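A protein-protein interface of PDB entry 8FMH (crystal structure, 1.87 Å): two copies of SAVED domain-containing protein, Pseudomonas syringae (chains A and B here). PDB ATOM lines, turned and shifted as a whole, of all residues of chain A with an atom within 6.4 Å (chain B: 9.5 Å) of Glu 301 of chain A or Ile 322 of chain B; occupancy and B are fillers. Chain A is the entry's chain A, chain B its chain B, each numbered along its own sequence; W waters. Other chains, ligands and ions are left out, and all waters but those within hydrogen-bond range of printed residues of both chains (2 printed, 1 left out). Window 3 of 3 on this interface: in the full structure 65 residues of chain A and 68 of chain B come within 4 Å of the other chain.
The side-chain amide oxygen (OE1) of Gln 321 of chain B sits at hydrogen-bond distance from the backbone NH (N) of Tyr 304 of chain A, at 2.9 Å.
Among the printed residues, pairs that only touch across the chains: Glu 301 of chain A with Ile 322 of chain B (3.3 Å), Pro 302 of chain A with Ile 322 of chain B (3.9 Å), Ser 303 of chain A with Gln 321 of chain B (3.4 Å), Ser 303 of chain A with Ile 322 of chain B (3.7 Å) and Tyr 304 of chain A with Leu 352 of chain B (3.8 Å).
Of the 8 printed residues of chain A, 4 touch a printed residue of chain B. Hydrophobic or aromatic side chains of chain A that line the printed part of chain B: Tyr 304. Of the 22 printed residues of chain B, 3 touch a printed residue of chain A. Among the printed residues, no Asp or Glu carboxylate lies within 4 Å of a Lys or Arg side-chain nitrogen of the other chain.
Water W1 lies within hydrogen-bond range of O of Ile 322 of chain B (2.6 Å) and O of Pro 302 of chain A (2.8 Å). Water W2 lies within hydrogen-bond range of OH of Tyr 304 of chain A (2.6 Å) and O of Leu 352 of chain B (2.7 Å).
No position is printed for both chains.
The backbone carbonyl oxygen of Ile 276 of chain A lies within hydrogen-bond range of the backbone NH of Ser 303 of chain A (3.0 Å).
Glu 301 of chain A touches one residue of chain B. Ile 322 of chain B touches three residues of chain A. Pro 300 of chain A touches none of the printed residues of chain B. Of chain B, only Gln 321 (3.4 Å) and Ile 322 (3.7 Å) come within 4 Å of Ser 303 of chain A. Of the printed residues of chain A, Leu 352 of chain B touches Tyr 304 (3.8 Å). Of the printed residues of chain A, Gln 321 of chain B touches Ser 303 (3.4 Å) and Tyr 304 (2.9 Å). Of the printed residues of chain B, Tyr 304 of chain A touches Gln 321 (2.9 Å) and Leu 352 (3.8 Å). Arg 317 of chain B touches none of the printed residues of chain A. The nearest residue of chain B that does not touch Glu 301 of chain A is Arg 323 of chain B (5.2 Å). The nearest residue of chain A that does not touch Ile 322 of chain B is Tyr 304 of chain A (5.8 Å).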
ATOM      1  N   ILE A 276     -23.264  15.135  -0.650  1.00  0.00           N
ATOM      2  CA  ILE A 276     -24.086  16.245  -1.120  1.00  0.00           C
ATOM      3  C   ILE A 276     -23.362  17.058  -2.186  1.00  0.00           C
ATOM      4  O   ILE A 276     -23.893  17.277  -3.281  1.00  0.00           O
ATOM      5  CB  ILE A 276     -24.534  17.144   0.055  1.00  0.00           C
ATOM      6  CG1 ILE A 276     -25.340  16.302   1.050  1.00  0.00           C
ATOM      7  CG2 ILE A 276     -25.370  18.327  -0.446  1.00  0.00           C
ATOM      8  CD1 ILE A 276     -25.765  17.031   2.291  1.00  0.00           C
ATOM      9  N   ILE A 299     -28.019  13.344  -2.228  1.00  0.00           N
ATOM     10  CA  ILE A 299     -29.029  13.862  -3.147  1.00  0.00           C
ATOM     11  C   ILE A 299     -28.842  13.170  -4.492  1.00  0.00           C
ATOM     12  O   ILE A 299     -27.767  12.621  -4.782  1.00  0.00           O
ATOM     13  CB  ILE A 299     -28.949  15.402  -3.281  1.00  0.00           C
ATOM     14  CG1 ILE A 299     -27.597  15.837  -3.849  1.00  0.00           C
ATOM     15  CG2 ILE A 299     -29.197  16.060  -1.923  1.00  0.00           C
ATOM     16  CD1 ILE A 299     -27.481  17.339  -4.102  1.00  0.00           C
ATOM     17  N   PRO A 300     -29.879  13.162  -5.331  1.00  0.00           N
ATOM     18  CA  PRO A 300     -29.773  12.437  -6.610  1.00  0.00           C
ATOM     19  C   PRO A 300     -28.564  12.822  -7.447  1.00  0.00           C
ATOM     20  O   PRO A 300     -27.884  11.936  -7.982  1.00  0.00           O
ATOM     21  CB  PRO A 300     -31.092  12.792  -7.306  1.00  0.00           C
ATOM     22  CG  PRO A 300     -32.054  12.999  -6.174  1.00  0.00           C
ATOM     23  CD  PRO A 300     -31.249  13.644  -5.080  1.00  0.00           C
ATOM     24  N   GLU A 301     -28.282  14.121  -7.583  1.00  0.00           N
ATOM     25  CA  GLU A 301     -27.128  14.627  -8.328  1.00  0.00           C
ATOM     26  C   GLU A 301     -26.269  15.456  -7.382  1.00  0.00           C
ATOM     27  O   GLU A 301     -26.448  16.680  -7.279  1.00  0.00           O
ATOM     28  CB  GLU A 301     -27.571  15.465  -9.526  1.00  0.00           C
ATOM     29  CG  GLU A 301     -27.232  14.873 -10.883  1.00  0.00           C
ATOM     30  CD  GLU A 301     -27.605  15.805 -12.024  1.00  0.00           C
ATOM     31  OE1 GLU A 301     -27.561  17.037 -11.822  1.00  0.00           O
ATOM     32  OE2 GLU A 301     -27.949  15.305 -13.117  1.00  0.00           O
ATOM     33  N   PRO A 302     -25.331  14.839  -6.666  1.00  0.00           N
ATOM     34  CA  PRO A 302     -24.414  15.623  -5.829  1.00  0.00           C
ATOM     35  C   PRO A 302     -23.692  16.674  -6.660  1.00  0.00           C
ATOM     36  O   PRO A 302     -23.098  16.369  -7.696  1.00  0.00           O
ATOM     37  CB  PRO A 302     -23.448  14.566  -5.276  1.00  0.00           C
ATOM     38  CG  PRO A 302     -24.200  13.284  -5.347  1.00  0.00           C
ATOM     39  CD  PRO A 302     -25.076  13.392  -6.561  1.00  0.00           C
ATOM     40  N   SER A 303     -23.747  17.925  -6.200  1.00  0.00           N
ATOM     41  CA  SER A 303     -23.186  19.034  -6.957  1.00  0.00           C
ATOM     42  C   SER A 303     -22.639  20.099  -6.019  1.00  0.00           C
ATOM     43  O   SER A 303     -23.220  20.368  -4.962  1.00  0.00           O
ATOM     44  CB  SER A 303     -24.235  19.665  -7.880  1.00  0.00           C
ATOM     45  OG  SER A 303     -23.642  20.615  -8.750  1.00  0.00           O
ATOM     46  N   TYR A 304     -21.525  20.713  -6.435  1.00  0.00           N
ATOM     47  CA  TYR A 304     -20.977  21.862  -5.723  1.00  0.00           C
ATOM     48  C   TYR A 304     -21.942  23.041  -5.703  1.00  0.00           C
ATOM     49  O   TYR A 304     -21.874  23.879  -4.796  1.00  0.00           O
ATOM     50  CB  TYR A 304     -19.665  22.307  -6.378  1.00  0.00           C
ATOM     51  CG  TYR A 304     -18.446  21.461  -6.077  1.00  0.00           C
ATOM     52  CD1 TYR A 304     -18.548  20.236  -5.431  1.00  0.00           C
ATOM     53  CD2 TYR A 304     -17.185  21.900  -6.438  1.00  0.00           C
ATOM     54  CE1 TYR A 304     -17.425  19.477  -5.158  1.00  0.00           C
ATOM     55  CE2 TYR A 304     -16.066  21.153  -6.170  1.00  0.00           C
ATOM     56  CZ  TYR A 304     -16.185  19.946  -5.528  1.00  0.00           C
ATOM     57  OH  TYR A 304     -15.050  19.210  -5.267  1.00  0.00           O
ATOM     58  N   MET A 306     -25.276  23.208  -5.465  1.00  0.00           N
ATOM     59  CA  MET A 306     -26.632  22.850  -5.073  1.00  0.00           C
ATOM     60  C   MET A 306     -27.254  23.781  -4.040  1.00  0.00           C
ATOM     61  O   MET A 306     -28.417  23.569  -3.683  1.00  0.00           O
ATOM     62  CB  MET A 306     -26.650  21.417  -4.529  1.00  0.00           C
ATOM     63  CG  MET A 306     -25.898  21.229  -3.212  1.00  0.00           C
ATOM     64  SD  MET A 306     -26.798  21.770  -1.747  1.00  0.00           S
ATOM     65  CE  MET A 306     -28.172  20.626  -1.723  1.00  0.00           C
ATOM     66  N   PHE B 258     -24.391  19.806 -21.766  1.00  0.00           N
ATOM     67  CA  PHE B 258     -23.156  19.039 -21.687  1.00  0.00           C
ATOM     68  C   PHE B 258     -23.514  17.565 -21.569  1.00  0.00           C
ATOM     69  O   PHE B 258     -24.230  17.163 -20.644  1.00  0.00           O
ATOM     70  CB  PHE B 258     -22.297  19.523 -20.522  1.00  0.00           C
ATOM     71  CG  PHE B 258     -21.692  20.880 -20.763  1.00  0.00           C
ATOM     72  CD1 PHE B 258     -22.389  22.029 -20.439  1.00  0.00           C
ATOM     73  CD2 PHE B 258     -20.443  21.002 -21.356  1.00  0.00           C
ATOM     74  CE1 PHE B 258     -21.846  23.275 -20.678  1.00  0.00           C
ATOM     75  CE2 PHE B 258     -19.896  22.248 -21.598  1.00  0.00           C
ATOM     76  CZ  PHE B 258     -20.600  23.384 -21.260  1.00  0.00           C
ATOM     77  N   PHE B 260     -22.846  13.471 -21.361  1.00  0.00           N
ATOM     78  CA  PHE B 260     -21.935  12.559 -20.678  1.00  0.00           C
ATOM     79  C   PHE B 260     -22.206  11.127 -21.115  1.00  0.00           C
ATOM     80  O   PHE B 260     -23.324  10.621 -20.958  1.00  0.00           O
ATOM     81  CB  PHE B 260     -22.059  12.683 -19.158  1.00  0.00           C
ATOM     82  CG  PHE B 260     -21.148  11.751 -18.405  1.00  0.00           C
ATOM     83  CD1 PHE B 260     -19.787  11.988 -18.353  1.00  0.00           C
ATOM     84  CD2 PHE B 260     -21.653  10.637 -17.757  1.00  0.00           C
ATOM     85  CE1 PHE B 260     -18.944  11.132 -17.666  1.00  0.00           C
ATOM     86  CE2 PHE B 260     -20.813   9.781 -17.068  1.00  0.00           C
ATOM     87  CZ  PHE B 260     -19.458  10.030 -17.027  1.00  0.00           C
ATOM     88  N   LEU B 272     -11.226  10.257 -19.441  1.00  0.00           N
ATOM     89  CA  LEU B 272     -12.290  11.234 -19.640  1.00  0.00           C
ATOM     90  C   LEU B 272     -11.937  12.089 -20.846  1.00  0.00           C
ATOM     91  O   LEU B 272     -10.940  12.819 -20.822  1.00  0.00           O
ATOM     92  CB  LEU B 272     -12.476  12.112 -18.401  1.00  0.00           C
ATOM     93  CG  LEU B 272     -13.445  13.288 -18.573  1.00  0.00           C
ATOM     94  CD1 LEU B 272     -14.855  12.800 -18.887  1.00  0.00           C
ATOM     95  CD2 LEU B 272     -13.443  14.172 -17.333  1.00  0.00           C
ATOM     96  N   LEU B 297     -17.345  13.816 -21.934  1.00  0.00           N
ATOM     97  CA  LEU B 297     -18.178  15.006 -21.836  1.00  0.00           C
ATOM     98  C   LEU B 297     -18.083  15.781 -23.147  1.00  0.00           C
ATOM     99  O   LEU B 297     -16.987  15.956 -23.692  1.00  0.00           O
ATOM    100  CB  LEU B 297     -17.733  15.894 -20.665  1.00  0.00           C
ATOM    101  CG  LEU B 297     -18.777  16.882 -20.128  1.00  0.00           C
ATOM    102  CD1 LEU B 297     -19.836  16.169 -19.302  1.00  0.00           C
ATOM    103  CD2 LEU B 297     -18.118  17.976 -19.307  1.00  0.00           C
ATOM    104  N   HIS B 314     -19.367  28.689 -16.458  1.00  0.00           N
ATOM    105  CA  HIS B 314     -19.995  28.183 -15.243  1.00  0.00           C
ATOM    106  C   HIS B 314     -20.689  26.857 -15.510  1.00  0.00           C
ATOM    107  O   HIS B 314     -20.520  25.889 -14.759  1.00  0.00           O
ATOM    108  CB  HIS B 314     -21.003  29.197 -14.704  1.00  0.00           C
ATOM    109  CG  HIS B 314     -20.393  30.472 -14.212  1.00  0.00           C
ATOM    110  ND1 HIS B 314     -19.326  30.503 -13.341  1.00  0.00           N
ATOM    111  CD2 HIS B 314     -20.720  31.765 -14.450  1.00  0.00           C
ATOM    112  CE1 HIS B 314     -19.016  31.758 -13.072  1.00  0.00           C
ATOM    113  NE2 HIS B 314     -19.848  32.543 -13.731  1.00  0.00           N
ATOM    114  N   ALA B 315     -21.493  26.802 -16.575  1.00  0.00           N
ATOM    115  CA  ALA B 315     -22.243  25.589 -16.884  1.00  0.00           C
ATOM    116  C   ALA B 315     -21.317  24.417 -17.158  1.00  0.00           C
ATOM    117  O   ALA B 315     -21.653  23.271 -16.837  1.00  0.00           O
ATOM    118  CB  ALA B 315     -23.155  25.832 -18.085  1.00  0.00           C
ATOM    119  N   PHE B 316     -20.152  24.678 -17.758  1.00  0.00           N
ATOM    120  CA  PHE B 316     -19.188  23.611 -17.984  1.00  0.00           C
ATOM    121  C   PHE B 316     -18.644  23.089 -16.665  1.00  0.00           C
ATOM    122  O   PHE B 316     -18.418  21.881 -16.514  1.00  0.00           O
ATOM    123  CB  PHE B 316     -18.051  24.114 -18.874  1.00  0.00           C
ATOM    124  CG  PHE B 316     -16.832  23.223 -18.874  1.00  0.00           C
ATOM    125  CD1 PHE B 316     -16.831  22.020 -19.565  1.00  0.00           C
ATOM    126  CD2 PHE B 316     -15.681  23.601 -18.196  1.00  0.00           C
ATOM    127  CE1 PHE B 316     -15.707  21.204 -19.568  1.00  0.00           C
ATOM    128  CE2 PHE B 316     -14.555  22.789 -18.198  1.00  0.00           C
ATOM    129  CZ  PHE B 316     -14.569  21.591 -18.887  1.00  0.00           C
ATOM    130  N   ARG B 317     -18.414  23.986 -15.704  1.00  0.00           N
ATOM    131  CA  ARG B 317     -17.931  23.561 -14.395  1.00  0.00           C
ATOM    132  C   ARG B 317     -18.972  22.703 -13.693  1.00  0.00           C
ATOM    133  O   ARG B 317     -18.653  21.655 -13.121  1.00  0.00           O
ATOM    134  CB  ARG B 317     -17.585  24.781 -13.538  1.00  0.00           C
ATOM    135  CG  ARG B 317     -17.282  24.453 -12.068  1.00  0.00           C
ATOM    136  CD  ARG B 317     -17.829  25.516 -11.126  1.00  0.00           C
ATOM    137  NE  ARG B 317     -17.064  26.756 -11.222  1.00  0.00           N
ATOM    138  CZ  ARG B 317     -17.580  27.957 -11.439  1.00  0.00           C
ATOM    139  NH1 ARG B 317     -18.890  28.151 -11.519  1.00  0.00           N
ATOM    140  NH2 ARG B 317     -16.759  28.997 -11.563  1.00  0.00           N
ATOM    141  N   ASP B 318     -20.223  23.152 -13.703  1.00  0.00           N
ATOM    142  CA  ASP B 318     -21.267  22.426 -12.996  1.00  0.00           C
ATOM    143  C   ASP B 318     -21.449  21.029 -13.580  1.00  0.00           C
ATOM    144  O   ASP B 318     -21.488  20.039 -12.844  1.00  0.00           O
ATOM    145  CB  ASP B 318     -22.566  23.227 -13.043  1.00  0.00           C
ATOM    146  CG  ASP B 318     -22.490  24.502 -12.219  1.00  0.00           C
ATOM    147  OD1 ASP B 318     -21.446  24.731 -11.569  1.00  0.00           O
ATOM    148  OD2 ASP B 318     -23.472  25.276 -12.215  1.00  0.00           O
ATOM    149  N   ALA B 319     -21.533  20.927 -14.910  1.00  0.00           N
ATOM    150  CA  ALA B 319     -21.628  19.615 -15.546  1.00  0.00           C
ATOM    151  C   ALA B 319     -20.378  18.787 -15.277  1.00  0.00           C
ATOM    152  O   ALA B 319     -20.462  17.615 -14.894  1.00  0.00           O
ATOM    153  CB  ALA B 319     -21.849  19.779 -17.050  1.00  0.00           C
ATOM    154  N   LEU B 320     -19.204  19.385 -15.471  1.00  0.00           N
ATOM    155  CA  LEU B 320     -17.962  18.638 -15.292  1.00  0.00           C
ATOM    156  C   LEU B 320     -17.852  18.072 -13.879  1.00  0.00           C
ATOM    157  O   LEU B 320     -17.496  16.902 -13.696  1.00  0.00           O
ATOM    158  CB  LEU B 320     -16.768  19.536 -15.608  1.00  0.00           C
ATOM    159  CG  LEU B 320     -15.376  18.943 -15.363  1.00  0.00           C
ATOM    160  CD1 LEU B 320     -15.076  17.854 -16.372  1.00  0.00           C
ATOM    161  CD2 LEU B 320     -14.324  20.033 -15.425  1.00  0.00           C
ATOM    162  N   GLN B 321     -18.160  18.884 -12.863  1.00  0.00           N
ATOM    163  CA  GLN B 321     -18.000  18.416 -11.491  1.00  0.00           C
ATOM    164  C   GLN B 321     -19.000  17.314 -11.167  1.00  0.00           C
ATOM    165  O   GLN B 321     -18.679  16.378 -10.427  1.00  0.00           O
ATOM    166  CB  GLN B 321     -18.150  19.579 -10.509  1.00  0.00           C
ATOM    167  CG  GLN B 321     -17.825  19.207  -9.073  1.00  0.00           C
ATOM    168  CD  GLN B 321     -19.020  18.671  -8.306  1.00  0.00           C
ATOM    169  OE1 GLN B 321     -20.137  19.179  -8.433  1.00  0.00           O
ATOM    170  NE2 GLN B 321     -18.790  17.640  -7.500  1.00  0.00           N
ATOM    171  N   ILE B 322     -20.217  17.408 -11.712  1.00  0.00           N
ATOM    172  CA  ILE B 322     -21.221  16.382 -11.451  1.00  0.00           C
ATOM    173  C   ILE B 322     -20.738  15.025 -11.949  1.00  0.00           C
ATOM    174  O   ILE B 322     -20.991  13.991 -11.314  1.00  0.00           O
ATOM    175  CB  ILE B 322     -22.566  16.784 -12.082  1.00  0.00           C
ATOM    176  CG1 ILE B 322     -23.171  17.941 -11.287  1.00  0.00           C
ATOM    177  CG2 ILE B 322     -23.531  15.602 -12.110  1.00  0.00           C
ATOM    178  CD1 ILE B 322     -24.558  18.375 -11.738  1.00  0.00           C
ATOM    179  N   ARG B 323     -20.029  15.003 -13.079  1.00  0.00           N
ATOM    180  CA  ARG B 323     -19.557  13.745 -13.645  1.00  0.00           C
ATOM    181  C   ARG B 323     -18.236  13.294 -13.042  1.00  0.00           C
ATOM    182  O   ARG B 323     -18.012  12.089 -12.896  1.00  0.00           O
ATOM    183  CB  ARG B 323     -19.399  13.856 -15.162  1.00  0.00           C
ATOM    184  CG  ARG B 323     -20.627  14.362 -15.898  1.00  0.00           C
ATOM    185  CD  ARG B 323     -21.862  13.561 -15.550  1.00  0.00           C
ATOM    186  NE  ARG B 323     -23.010  13.988 -16.336  1.00  0.00           N
ATOM    187  CZ  ARG B 323     -24.131  13.292 -16.456  1.00  0.00           C
ATOM    188  NH1 ARG B 323     -24.276  12.115 -15.874  1.00  0.00           N
ATOM    189  NH2 ARG B 323     -25.127  13.787 -17.187  1.00  0.00           N
ATOM    190  N   LEU B 324     -17.346  14.227 -12.704  1.00  0.00           N
ATOM    191  CA  LEU B 324     -16.116  13.835 -12.029  1.00  0.00           C
ATOM    192  C   LEU B 324     -16.429  13.162 -10.701  1.00  0.00           C
ATOM    193  O   LEU B 324     -15.739  12.221 -10.293  1.00  0.00           O
ATOM    194  CB  LEU B 324     -15.214  15.050 -11.818  1.00  0.00           C
ATOM    195  CG  LEU B 324     -14.615  15.734 -13.050  1.00  0.00           C
ATOM    196  CD1 LEU B 324     -13.638  16.829 -12.619  1.00  0.00           C
ATOM    197  CD2 LEU B 324     -13.925  14.737 -13.970  1.00  0.00           C
ATOM    198  N   SER B 325     -17.474  13.627 -10.014  1.00  0.00           N
ATOM    199  CA  SER B 325     -17.911  12.954  -8.797  1.00  0.00           C
ATOM    200  C   SER B 325     -18.286  11.507  -9.087  1.00  0.00           C
ATOM    201  O   SER B 325     -17.923  10.600  -8.328  1.00  0.00           O
ATOM    202  CB  SER B 325     -19.093  13.699  -8.176  1.00  0.00           C
ATOM    203  OG  SER B 325     -19.612  12.995  -7.058  1.00  0.00           O
ATOM    204  N   GLN B 326     -19.012  11.274 -10.184  1.00  0.00           N
ATOM    205  CA  GLN B 326     -19.319   9.909 -10.594  1.00  0.00           C
ATOM    206  C   GLN B 326     -18.045   9.138 -10.908  1.00  0.00           C
ATOM    207  O   GLN B 326     -17.840   8.022 -10.416  1.00  0.00           O
ATOM    208  CB  GLN B 326     -20.238   9.927 -11.814  1.00  0.00           C
ATOM    209  CG  GLN B 326     -21.613  10.526 -11.557  1.00  0.00           C
ATOM    210  CD  GLN B 326     -22.425  10.708 -12.830  1.00  0.00           C
ATOM    211  OE1 GLN B 326     -23.277  11.591 -12.907  1.00  0.00           O
ATOM    212  NE2 GLN B 326     -22.171   9.871 -13.829  1.00  0.00           N
ATOM    213  N   LEU B 327     -17.170   9.725 -11.726  1.00  0.00           N
ATOM    214  CA  LEU B 327     -15.956   9.027 -12.129  1.00  0.00           C
ATOM    215  C   LEU B 327     -15.012   8.816 -10.952  1.00  0.00           C
ATOM    216  O   LEU B 327     -14.346   7.777 -10.865  1.00  0.00           O
ATOM    217  CB  LEU B 327     -15.253   9.800 -13.242  1.00  0.00           C
ATOM    218  CG  LEU B 327     -16.067   9.995 -14.520  1.00  0.00           C
ATOM    219  CD1 LEU B 327     -15.268  10.837 -15.497  1.00  0.00           C
ATOM    220  CD2 LEU B 327     -16.461   8.650 -15.141  1.00  0.00           C
ATOM    221  N   GLU B 328     -14.931   9.785 -10.038  1.00  0.00           N
ATOM    222  CA  GLU B 328     -14.037   9.621  -8.898  1.00  0.00           C
ATOM    223  C   GLU B 328     -14.501   8.499  -7.975  1.00  0.00           C
ATOM    224  O   GLU B 328     -13.668   7.796  -7.392  1.00  0.00           O
ATOM    225  CB  GLU B 328     -13.912  10.938  -8.135  1.00  0.00           C
ATOM    226  CG  GLU B 328     -13.023  11.954  -8.850  1.00  0.00           C
ATOM    227  CD  GLU B 328     -12.808  13.235  -8.060  1.00  0.00           C
ATOM    228  OE1 GLU B 328     -13.272  13.309  -6.902  1.00  0.00           O
ATOM    229  OE2 GLU B 328     -12.174  14.167  -8.607  1.00  0.00           O
ATOM    230  N   ALA B 329     -15.813   8.305  -7.838  1.00  0.00           N
ATOM    231  CA  ALA B 329     -16.345   7.236  -7.001  1.00  0.00           C
ATOM    232  C   ALA B 329     -16.251   5.861  -7.654  1.00  0.00           C
ATOM    233  O   ALA B 329     -16.468   4.854  -6.969  1.00  0.00           O
ATOM    234  CB  ALA B 329     -17.805   7.528  -6.642  1.00  0.00           C
ATOM    235  N   LEU B 352     -11.391  24.273 -10.621  1.00  0.00           N
ATOM    236  CA  LEU B 352     -12.309  23.374  -9.935  1.00  0.00           C
ATOM    237  C   LEU B 352     -11.559  22.418  -9.017  1.00  0.00           C
ATOM    238  O   LEU B 352     -12.006  22.135  -7.898  1.00  0.00           O
ATOM    239  CB  LEU B 352     -13.121  22.601 -10.970  1.00  0.00           C
ATOM    240  CG  LEU B 352     -14.111  21.569 -10.450  1.00  0.00           C
ATOM    241  CD1 LEU B 352     -15.269  22.264  -9.736  1.00  0.00           C
ATOM    242  CD2 LEU B 352     -14.588  20.719 -11.619  1.00  0.00           C
ATOM    243  N   TYR B 361      -5.371  12.990 -11.205  1.00  0.00           N
ATOM    244  CA  TYR B 361      -5.669  13.222 -12.613  1.00  0.00           C
ATOM    245  C   TYR B 361      -4.357  13.285 -13.379  1.00  0.00           C
ATOM    246  O   TYR B 361      -3.414  13.958 -12.948  1.00  0.00           O
ATOM    247  CB  TYR B 361      -6.453  14.524 -12.824  1.00  0.00           C
ATOM    248  CG  TYR B 361      -7.889  14.447 -12.372  1.00  0.00           C
ATOM    249  CD1 TYR B 361      -8.223  14.628 -11.041  1.00  0.00           C
ATOM    250  CD2 TYR B 361      -8.911  14.190 -13.274  1.00  0.00           C
ATOM    251  CE1 TYR B 361      -9.533  14.556 -10.619  1.00  0.00           C
ATOM    252  CE2 TYR B 361     -10.225  14.117 -12.860  1.00  0.00           C
ATOM    253  CZ  TYR B 361     -10.528  14.299 -11.530  1.00  0.00           C
ATOM    254  OH  TYR B 361     -11.831  14.225 -11.098  1.00  0.00           O
HETATM  255  O   HOH W   1     -22.630  14.140  -9.354  1.00  0.00           O
HETATM  256  O   HOH W   2     -12.974  19.871  -6.730  1.00  0.00           O
